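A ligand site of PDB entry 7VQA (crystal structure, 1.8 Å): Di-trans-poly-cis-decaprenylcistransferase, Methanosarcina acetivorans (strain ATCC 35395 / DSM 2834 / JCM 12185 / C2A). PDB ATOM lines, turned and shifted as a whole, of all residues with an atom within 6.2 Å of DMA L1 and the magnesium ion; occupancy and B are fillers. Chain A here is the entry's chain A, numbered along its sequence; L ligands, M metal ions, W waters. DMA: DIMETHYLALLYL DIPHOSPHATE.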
ATOM      1  N   PRO A  22     -13.929  -1.172   6.021  1.00  0.00           N
ATOM      2  CA  PRO A  22     -14.393  -2.561   5.891  1.00  0.00           C
ATOM      3  C   PRO A  22     -15.462  -2.650   4.776  1.00  0.00           C
ATOM      4  O   PRO A  22     -16.607  -2.917   5.078  1.00  0.00           O
ATOM      5  CB  PRO A  22     -14.990  -2.852   7.279  1.00  0.00           C
ATOM      6  CG  PRO A  22     -15.563  -1.503   7.666  1.00  0.00           C
ATOM      7  CD  PRO A  22     -14.560  -0.480   7.163  1.00  0.00           C
ATOM      8  N   ASP A  23     -15.058  -2.323   3.549  1.00  0.00           N
ATOM      9  CA  ASP A  23     -15.999  -2.189   2.416  1.00  0.00           C
ATOM     10  C   ASP A  23     -16.256  -3.538   1.755  1.00  0.00           C
ATOM     11  O   ASP A  23     -15.402  -4.456   1.820  1.00  0.00           O
ATOM     12  CB  ASP A  23     -15.505  -1.163   1.407  1.00  0.00           C
ATOM     13  CG  ASP A  23     -16.456  -0.673   0.333  1.00  0.00           C
ATOM     14  OD1 ASP A  23     -17.673  -0.470   0.626  1.00  0.00           O
ATOM     15  OD2 ASP A  23     -15.965  -0.413  -0.821  1.00  0.00           O
ATOM     16  N   GLY A  24     -17.395  -3.626   1.063  1.00  0.00           N
ATOM     17  CA  GLY A  24     -17.689  -4.756   0.155  1.00  0.00           C
ATOM     18  C   GLY A  24     -18.690  -5.753   0.743  1.00  0.00           C
ATOM     19  O   GLY A  24     -18.840  -6.805   0.197  1.00  0.00           O
ATOM     20  N   ASN A  25     -19.394  -5.428   1.809  1.00  0.00           N
ATOM     21  CA  ASN A  25     -20.328  -6.393   2.432  1.00  0.00           C
ATOM     22  C   ASN A  25     -21.503  -6.741   1.488  1.00  0.00           C
ATOM     23  O   ASN A  25     -21.889  -7.909   1.475  1.00  0.00           O
ATOM     24  CB  ASN A  25     -20.858  -5.850   3.751  1.00  0.00           C
ATOM     25  CG  ASN A  25     -19.722  -5.545   4.720  1.00  0.00           C
ATOM     26  OD1 ASN A  25     -19.028  -6.454   5.161  1.00  0.00           O
ATOM     27  ND2 ASN A  25     -19.420  -4.278   4.938  1.00  0.00           N
ATOM     28  N   ARG A  26     -22.077  -5.776   0.777  1.00  0.00           N
ATOM     29  CA  ARG A  26     -23.253  -6.051  -0.101  1.00  0.00           C
ATOM     30  C   ARG A  26     -22.797  -6.915  -1.283  1.00  0.00           C
ATOM     31  O   ARG A  26     -23.475  -7.940  -1.619  1.00  0.00           O
ATOM     32  CB  ARG A  26     -23.939  -4.749  -0.513  1.00  0.00           C
ATOM     33  CG  ARG A  26     -24.488  -3.931   0.657  1.00  0.00           C
ATOM     34  CD  ARG A  26     -25.203  -2.714   0.161  1.00  0.00           C
ATOM     35  NE  ARG A  26     -24.436  -1.828  -0.678  1.00  0.00           N
ATOM     36  CZ  ARG A  26     -24.907  -0.678  -1.199  1.00  0.00           C
ATOM     37  NH1 ARG A  26     -26.156  -0.301  -0.977  1.00  0.00           N
ATOM     38  NH2 ARG A  26     -24.126   0.091  -1.950  1.00  0.00           N
ATOM     39  N   ARG A  27     -21.658  -6.586  -1.903  1.00  0.00           N
ATOM     40  CA  ARG A  27     -21.131  -7.384  -3.007  1.00  0.00           C
ATOM     41  C   ARG A  27     -20.883  -8.807  -2.528  1.00  0.00           C
ATOM     42  O   ARG A  27     -21.194  -9.751  -3.287  1.00  0.00           O
ATOM     43  CB  ARG A  27     -19.849  -6.781  -3.596  1.00  0.00           C
ATOM     44  CG  ARG A  27     -20.164  -5.604  -4.507  1.00  0.00           C
ATOM     45  CD  ARG A  27     -18.880  -4.887  -4.824  1.00  0.00           C
ATOM     46  NE  ARG A  27     -18.518  -3.991  -3.709  1.00  0.00           N
ATOM     47  CZ  ARG A  27     -17.314  -3.449  -3.563  1.00  0.00           C
ATOM     48  NH1 ARG A  27     -16.367  -3.685  -4.450  1.00  0.00           N
ATOM     49  NH2 ARG A  27     -17.057  -2.655  -2.515  1.00  0.00           N
ATOM     50  N   TRP A  28     -20.277  -8.950  -1.345  1.00  0.00           N
ATOM     51  CA  TRP A  28     -19.924 -10.266  -0.763  1.00  0.00           C
ATOM     52  C   TRP A  28     -21.206 -11.104  -0.621  1.00  0.00           C
ATOM     53  O   TRP A  28     -21.219 -12.249  -1.079  1.00  0.00           O
ATOM     54  CB  TRP A  28     -19.227 -10.073   0.565  1.00  0.00           C
ATOM     55  CG  TRP A  28     -18.843 -11.354   1.215  1.00  0.00           C
ATOM     56  CD1 TRP A  28     -17.699 -12.061   1.006  1.00  0.00           C
ATOM     57  CD2 TRP A  28     -19.672 -12.164   2.064  1.00  0.00           C
ATOM     58  NE1 TRP A  28     -17.699 -13.184   1.801  1.00  0.00           N
ATOM     59  CE2 TRP A  28     -18.904 -13.286   2.427  1.00  0.00           C
ATOM     60  CE3 TRP A  28     -20.942 -12.006   2.598  1.00  0.00           C
ATOM     61  CZ2 TRP A  28     -19.405 -14.278   3.267  1.00  0.00           C
ATOM     62  CZ3 TRP A  28     -21.424 -12.974   3.443  1.00  0.00           C
ATOM     63  CH2 TRP A  28     -20.643 -14.084   3.790  1.00  0.00           C
ATOM     64  N   TYR A  40     -23.704  -7.662   6.264  1.00  0.00           N
ATOM     65  CA  TYR A  40     -23.163  -6.883   7.425  1.00  0.00           C
ATOM     66  C   TYR A  40     -22.884  -7.804   8.610  1.00  0.00           C
ATOM     67  O   TYR A  40     -21.832  -7.662   9.251  1.00  0.00           O
ATOM     68  CB  TYR A  40     -24.077  -5.734   7.822  1.00  0.00           C
ATOM     69  CG  TYR A  40     -24.191  -4.770   6.696  1.00  0.00           C
ATOM     70  CD1 TYR A  40     -23.089  -4.110   6.180  1.00  0.00           C
ATOM     71  CD2 TYR A  40     -25.419  -4.559   6.107  1.00  0.00           C
ATOM     72  CE1 TYR A  40     -23.232  -3.231   5.113  1.00  0.00           C
ATOM     73  CE2 TYR A  40     -25.584  -3.698   5.056  1.00  0.00           C
ATOM     74  CZ  TYR A  40     -24.486  -3.051   4.533  1.00  0.00           C
ATOM     75  OH  TYR A  40     -24.706  -2.234   3.474  1.00  0.00           O
ATOM     76  N   GLY A  66     -17.300   2.787  10.354  1.00  0.00           N
ATOM     77  CA  GLY A  66     -18.569   2.052  10.547  1.00  0.00           C
ATOM     78  C   GLY A  66     -19.572   2.412   9.462  1.00  0.00           C
ATOM     79  O   GLY A  66     -19.986   1.530   8.703  1.00  0.00           O
ATOM     80  N   PHE A  67     -20.144   3.620   9.518  1.00  0.00           N
ATOM     81  CA  PHE A  67     -21.019   4.093   8.426  1.00  0.00           C
ATOM     82  C   PHE A  67     -21.107   5.604   8.414  1.00  0.00           C
ATOM     83  O   PHE A  67     -20.869   6.276   9.447  1.00  0.00           O
ATOM     84  CB  PHE A  67     -22.412   3.469   8.538  1.00  0.00           C
ATOM     85  CG  PHE A  67     -23.255   3.945   9.695  1.00  0.00           C
ATOM     86  CD1 PHE A  67     -24.021   5.089   9.617  1.00  0.00           C
ATOM     87  CD2 PHE A  67     -23.301   3.202  10.868  1.00  0.00           C
ATOM     88  CE1 PHE A  67     -24.868   5.459  10.652  1.00  0.00           C
ATOM     89  CE2 PHE A  67     -24.158   3.566  11.889  1.00  0.00           C
ATOM     90  CZ  PHE A  67     -24.924   4.705  11.775  1.00  0.00           C
ATOM     91  N   THR A  68     -21.420   6.153   7.240  1.00  0.00           N
ATOM     92  CA  THR A  68     -21.497   7.602   6.989  1.00  0.00           C
ATOM     93  C   THR A  68     -22.947   8.063   7.061  1.00  0.00           C
ATOM     94  O   THR A  68     -23.864   7.246   7.030  1.00  0.00           O
ATOM     95  CB  THR A  68     -20.946   7.982   5.610  1.00  0.00           C
ATOM     96  OG1 THR A  68     -21.741   7.317   4.618  1.00  0.00           O
ATOM     97  CG2 THR A  68     -19.506   7.565   5.412  1.00  0.00           C
ATOM     98  N   ASN A  71     -24.581   6.912   3.983  1.00  0.00           N
ATOM     99  CA  ASN A  71     -25.019   5.501   4.049  1.00  0.00           C
ATOM    100  C   ASN A  71     -26.443   5.384   4.575  1.00  0.00           C
ATOM    101  O   ASN A  71     -27.112   4.419   4.174  1.00  0.00           O
ATOM    102  CB  ASN A  71     -24.104   4.645   4.906  1.00  0.00           C
ATOM    103  CG  ASN A  71     -22.756   4.379   4.274  1.00  0.00           C
ATOM    104  OD1 ASN A  71     -22.587   4.386   3.020  1.00  0.00           O
ATOM    105  ND2 ASN A  71     -21.766   4.193   5.115  1.00  0.00           N
ATOM    106  N   ARG A  74     -29.536   4.890   2.351  1.00  0.00           N
ATOM    107  CA  ARG A  74     -29.771   3.557   1.780  1.00  0.00           C
ATOM    108  C   ARG A  74     -31.121   3.023   2.252  1.00  0.00           C
ATOM    109  O   ARG A  74     -31.719   3.521   3.194  1.00  0.00           O
ATOM    110  CB  ARG A  74     -28.632   2.613   2.137  1.00  0.00           C
ATOM    111  CG  ARG A  74     -27.352   2.976   1.414  1.00  0.00           C
ATOM    112  CD  ARG A  74     -26.285   1.981   1.799  1.00  0.00           C
ATOM    113  NE  ARG A  74     -25.026   2.254   1.155  1.00  0.00           N
ATOM    114  CZ  ARG A  74     -23.969   1.479   1.304  1.00  0.00           C
ATOM    115  NH1 ARG A  74     -24.062   0.460   2.127  1.00  0.00           N
ATOM    116  NH2 ARG A  74     -22.814   1.779   0.738  1.00  0.00           N
ATOM    117  N   GLN A  78     -31.308  -2.201   4.761  1.00  0.00           N
ATOM    118  CA  GLN A  78     -29.818  -2.176   4.760  1.00  0.00           C
ATOM    119  C   GLN A  78     -29.330  -1.373   5.971  1.00  0.00           C
ATOM    120  O   GLN A  78     -28.461  -1.870   6.713  1.00  0.00           O
ATOM    121  CB  GLN A  78     -29.286  -1.568   3.473  1.00  0.00           C
ATOM    122  CG  GLN A  78     -29.523  -2.455   2.279  1.00  0.00           C
ATOM    123  CD  GLN A  78     -28.991  -1.830   1.007  1.00  0.00           C
ATOM    124  OE1 GLN A  78     -27.989  -1.135   1.031  1.00  0.00           O
ATOM    125  NE2 GLN A  78     -29.693  -2.019  -0.093  1.00  0.00           N
ATOM    126  N   PHE A  82     -26.854  -2.714   8.930  1.00  0.00           N
ATOM    127  CA  PHE A  82     -25.450  -2.255   9.120  1.00  0.00           C
ATOM    128  C   PHE A  82     -25.343  -1.613  10.504  1.00  0.00           C
ATOM    129  O   PHE A  82     -24.288  -1.743  11.167  1.00  0.00           O
ATOM    130  CB  PHE A  82     -24.874  -1.411   7.976  1.00  0.00           C
ATOM    131  CG  PHE A  82     -25.446  -0.047   7.651  1.00  0.00           C
ATOM    132  CD1 PHE A  82     -25.386   1.018   8.536  1.00  0.00           C
ATOM    133  CD2 PHE A  82     -25.895   0.208   6.358  1.00  0.00           C
ATOM    134  CE1 PHE A  82     -25.870   2.268   8.162  1.00  0.00           C
ATOM    135  CE2 PHE A  82     -26.354   1.459   5.981  1.00  0.00           C
ATOM    136  CZ  PHE A  82     -26.353   2.486   6.880  1.00  0.00           C
ATOM    137  N   CYS A  86     -22.910  -2.823  13.443  1.00  0.00           N
ATOM    138  CA  CYS A  86     -21.985  -1.868  14.111  1.00  0.00           C
ATOM    139  C   CYS A  86     -22.156  -1.964  15.634  1.00  0.00           C
ATOM    140  O   CYS A  86     -21.161  -2.094  16.348  1.00  0.00           O
ATOM    141  CB  CYS A  86     -22.225  -0.434  13.667  1.00  0.00           C
ATOM    142  SG  CYS A  86     -21.634  -0.094  11.996  1.00  0.00           S
ATOM    143  N   ARG A 173      -7.973  -0.576   3.104  1.00  0.00           N
ATOM    144  CA  ARG A 173      -9.338  -0.682   2.582  1.00  0.00           C
ATOM    145  C   ARG A 173      -9.540  -2.022   1.900  1.00  0.00           C
ATOM    146  O   ARG A 173      -8.755  -2.342   1.024  1.00  0.00           O
ATOM    147  CB  ARG A 173      -9.610   0.504   1.659  1.00  0.00           C
ATOM    148  CG  ARG A 173     -10.970   0.442   1.030  1.00  0.00           C
ATOM    149  CD  ARG A 173     -11.333   1.781   0.414  1.00  0.00           C
ATOM    150  NE  ARG A 173     -12.704   1.678  -0.022  1.00  0.00           N
ATOM    151  CZ  ARG A 173     -13.600   2.634  -0.081  1.00  0.00           C
ATOM    152  NH1 ARG A 173     -13.311   3.848   0.338  1.00  0.00           N
ATOM    153  NH2 ARG A 173     -14.826   2.341  -0.475  1.00  0.00           N
ATOM    154  N   ARG A 177     -11.813  -0.806  -3.832  1.00  0.00           N
ATOM    155  CA  ARG A 177     -11.913   0.618  -4.244  1.00  0.00           C
ATOM    156  C   ARG A 177     -10.723   1.424  -3.677  1.00  0.00           C
ATOM    157  O   ARG A 177     -10.474   1.323  -2.492  1.00  0.00           O
ATOM    158  CB  ARG A 177     -13.254   1.227  -3.848  1.00  0.00           C
ATOM    159  CG  ARG A 177     -14.460   0.385  -4.228  1.00  0.00           C
ATOM    160  CD  ARG A 177     -14.782   0.491  -5.697  1.00  0.00           C
ATOM    161  NE  ARG A 177     -15.825  -0.444  -6.107  1.00  0.00           N
ATOM    162  CZ  ARG A 177     -15.957  -0.907  -7.341  1.00  0.00           C
ATOM    163  NH1 ARG A 177     -15.119  -0.522  -8.293  1.00  0.00           N
ATOM    164  NH2 ARG A 177     -16.924  -1.760  -7.630  1.00  0.00           N
ATOM    165  N   ARG A 179     -10.009   4.660  -2.690  1.00  0.00           N
ATOM    166  CA  ARG A 179     -10.560   5.982  -2.313  1.00  0.00           C
ATOM    167  C   ARG A 179     -10.796   6.027  -0.800  1.00  0.00           C
ATOM    168  O   ARG A 179     -10.805   4.972  -0.187  1.00  0.00           O
ATOM    169  CB  ARG A 179     -11.848   6.292  -3.064  1.00  0.00           C
ATOM    170  CG  ARG A 179     -12.923   5.220  -3.002  1.00  0.00           C
ATOM    171  CD  ARG A 179     -13.955   5.555  -4.070  1.00  0.00           C
ATOM    172  NE  ARG A 179     -15.137   4.708  -4.033  1.00  0.00           N
ATOM    173  CZ  ARG A 179     -15.663   4.101  -5.085  1.00  0.00           C
ATOM    174  NH1 ARG A 179     -15.116   4.238  -6.284  1.00  0.00           N
ATOM    175  NH2 ARG A 179     -16.735   3.356  -4.938  1.00  0.00           N
ATOM    176  N   MET A 199     -13.550  -8.589  -0.665  1.00  0.00           N
ATOM    177  CA  MET A 199     -14.529  -7.920   0.193  1.00  0.00           C
ATOM    178  C   MET A 199     -14.211  -8.165   1.666  1.00  0.00           C
ATOM    179  O   MET A 199     -13.657  -9.197   2.051  1.00  0.00           O
ATOM    180  CB  MET A 199     -15.945  -8.404  -0.167  1.00  0.00           C
ATOM    181  CG  MET A 199     -16.318  -8.267  -1.642  1.00  0.00           C
ATOM    182  SD  MET A 199     -16.160  -6.632  -2.396  1.00  0.00           S
ATOM    183  CE  MET A 199     -14.928  -6.950  -3.656  1.00  0.00           C
HETATM  184  C1  DMA L   1     -19.474  -1.284   3.572  1.00  0.00           C
HETATM  185  O1  DMA L   1     -19.984  -2.212   2.646  1.00  0.00           O
HETATM  186  C2  DMA L   1     -20.457  -1.039   4.670  1.00  0.00           C
HETATM  187  C3  DMA L   1     -21.106   0.086   4.827  1.00  0.00           C
HETATM  188  C4  DMA L   1     -21.972   0.358   6.025  1.00  0.00           C
HETATM  189  C5  DMA L   1     -21.054   1.196   3.819  1.00  0.00           C
HETATM  190  PA  DMA L   1     -21.100  -1.738   1.599  1.00  0.00           P
HETATM  191  O1A DMA L   1     -22.439  -1.819   2.229  1.00  0.00           O
HETATM  192  O2A DMA L   1     -20.697  -0.430   1.029  1.00  0.00           O
HETATM  193  O3A DMA L   1     -20.968  -2.866   0.467  1.00  0.00           O
HETATM  194  PB  DMA L   1     -20.650  -2.702  -1.102  1.00  0.00           P
HETATM  195  O1B DMA L   1     -20.413  -4.067  -1.619  1.00  0.00           O
HETATM  196  O2B DMA L   1     -21.860  -2.050  -1.691  1.00  0.00           O
HETATM  197  O3B DMA L   1     -19.447  -1.840  -1.206  1.00  0.00           O
HETATM  198  C1  DMA L   2     -17.166   3.053   2.451  1.00  0.00           C
HETATM  199  O1  DMA L   2     -18.468   3.588   2.292  1.00  0.00           O
HETATM  200  C2  DMA L   2     -17.144   2.021   3.531  1.00  0.00           C
HETATM  201  C3  DMA L   2     -17.595   2.137   4.766  1.00  0.00           C
HETATM  202  C4  DMA L   2     -18.241   3.385   5.281  1.00  0.00           C
HETATM  203  C5  DMA L   2     -17.493   1.025   5.755  1.00  0.00           C
HETATM  204  PA  DMA L   2     -19.183   3.483   0.868  1.00  0.00           P
HETATM  205  O1A DMA L   2     -19.153   2.076   0.391  1.00  0.00           O
HETATM  206  O2A DMA L   2     -20.487   4.176   1.041  1.00  0.00           O
HETATM  207  O3A DMA L   2     -18.244   4.405  -0.035  1.00  0.00           O
HETATM  208  PB  DMA L   2     -17.980   4.571  -1.604  1.00  0.00           P
HETATM  209  O1B DMA L   2     -19.302   4.651  -2.249  1.00  0.00           O
HETATM  210  O2B DMA L   2     -17.185   5.820  -1.733  1.00  0.00           O
HETATM  211  O3B DMA L   2     -17.218   3.367  -2.019  1.00  0.00           O
HETATM  212 MG    MG M   1     -19.384   0.273  -0.554  1.00  0.00          MG
HETATM  213  O   HOH W   1     -17.911   0.797  -2.003  1.00  0.00           O
HETATM  214  O   HOH W   2     -20.913   0.688  -1.799  1.00  0.00           O
HETATM  215  O   HOH W   3     -23.207  -3.154  -4.034  1.00  0.00           O
HETATM  216  O   HOH W   4     -21.200  -1.195  -4.600  1.00  0.00           O
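Arg 74 touches the magnesium ion (NH2 to MG, 3.96 Å).
Two residues have an atom within 4 Å of the magnesium ion: Asp 23 and Arg 74.
Along chain A the residues within 4 Å of the magnesium ion span positions 23 to 74.
The nearest printed residue that does not touch the magnesium ion is Arg 27 (4.2 Å).
OD2 of Asp 23 is in salt-bridge range of NH2 of Arg 27 (3.0 Å).
NH2 of Arg 173 is in salt-bridge range of OD2 of Asp 23.
The side-chain hydroxyl of Tyr 40 lies within hydrogen-bond range of the guanidinium group of Arg 74, at 3.1 Å.
The side-chain amide oxygen of Gln 78 sits at hydrogen-bond distance from the guanidinium group of Arg 26, at 2.8 Å.
NH2 of Arg 74 sits at hydrogen-bond distance from OD1 of Asn 71 (3.5 Å).
NH1 of Arg 27 sits close to SD of Met 199 (3.6 Å).
The backbone carbonyl oxygen (O) of Pro 22 is in hydrogen-bond range of the side-chain amide nitrogen (ND2) of Asn 25, 3.1 Å away.
O of Phe 82 is in hydrogen-bond range of SG of Cys 86 (3.2 Å).
Pro 22 touches DMA L1.
O of Gly 66 touches C4 of DMA L1, 3.5 Å away.
ND2 of Asn 71 touches C5 of DMA L1, at 3.3 Å.
Phe 82 touches DMA L1.
Hydrophobic or aromatic side chains within 4 Å of DMA L1: Tyr 40 and Phe 82.
11 residues have an atom within 4 Å of DMA L1: Pro 22, Asp 23, Gly 24, Asn 25, Arg 26, Arg 27, Tyr 40, Gly 66, Asn 71, Arg 74 and Phe 82.
The side-chain hydroxyl of Tyr 40 is in hydrogen-bond range of an oxygen (O1A) of DMA L1 (2.6 Å).
N of Arg 26 lies within hydrogen-bond range of O3A of DMA L1 (3.1 Å).
The guanidinium group of Arg 26 lies within salt-bridge range of an oxygen (O2B) of DMA L1, 2.8 Å away.
O1A of DMA L1 lies within salt-bridge range of NH1 of Arg 74 (2.8 Å).
N of Arg 27 sits at hydrogen-bond distance from O1B of DMA L1 (2.8 Å).
NE of Arg 27 is in salt-bridge range of O1B of DMA L1.
N of Asn 25 is in hydrogen-bond range of O3A of DMA L1, 3.3 Å away.
The side-chain amide nitrogen of Asn 25 lies within hydrogen-bond range of an oxygen (O1) of DMA L1 (3.1 Å).
O1 of DMA L1 sits at hydrogen-bond distance from N of Gly 24, at 3.3 Å.
O2A of DMA L2 is in salt-bridge range of NH2 of Arg 74 (3.4 Å).
The side-chain amide oxygen (OD1) of Asn 71 lies close to an oxygen (O2A) of DMA L2.
O3B of DMA L2 is in salt-bridge range of NH2 of Arg 173, 3.0 Å away.
O3B of DMA L2 is in salt-bridge range of NH2 of Arg 179 (3.0 Å).
The magnesium ion is bound by water W2, O1A of DMA L2, water W1, O2A of DMA L1, OD1 of Asp 23 and O3B of DMA L1.
The magnesium ion has six donor atoms within binding distance.
Water W2 lies within hydrogen-bond range of O2B of DMA L1, NH2 of Arg 26 and NH2 of Arg 74.
Water W1 lies within hydrogen-bond range of the side-chain carboxylate (OD2) of Asp 23 (2.6 Å) and an oxygen (O3B) of DMA L2 (2.7 Å).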
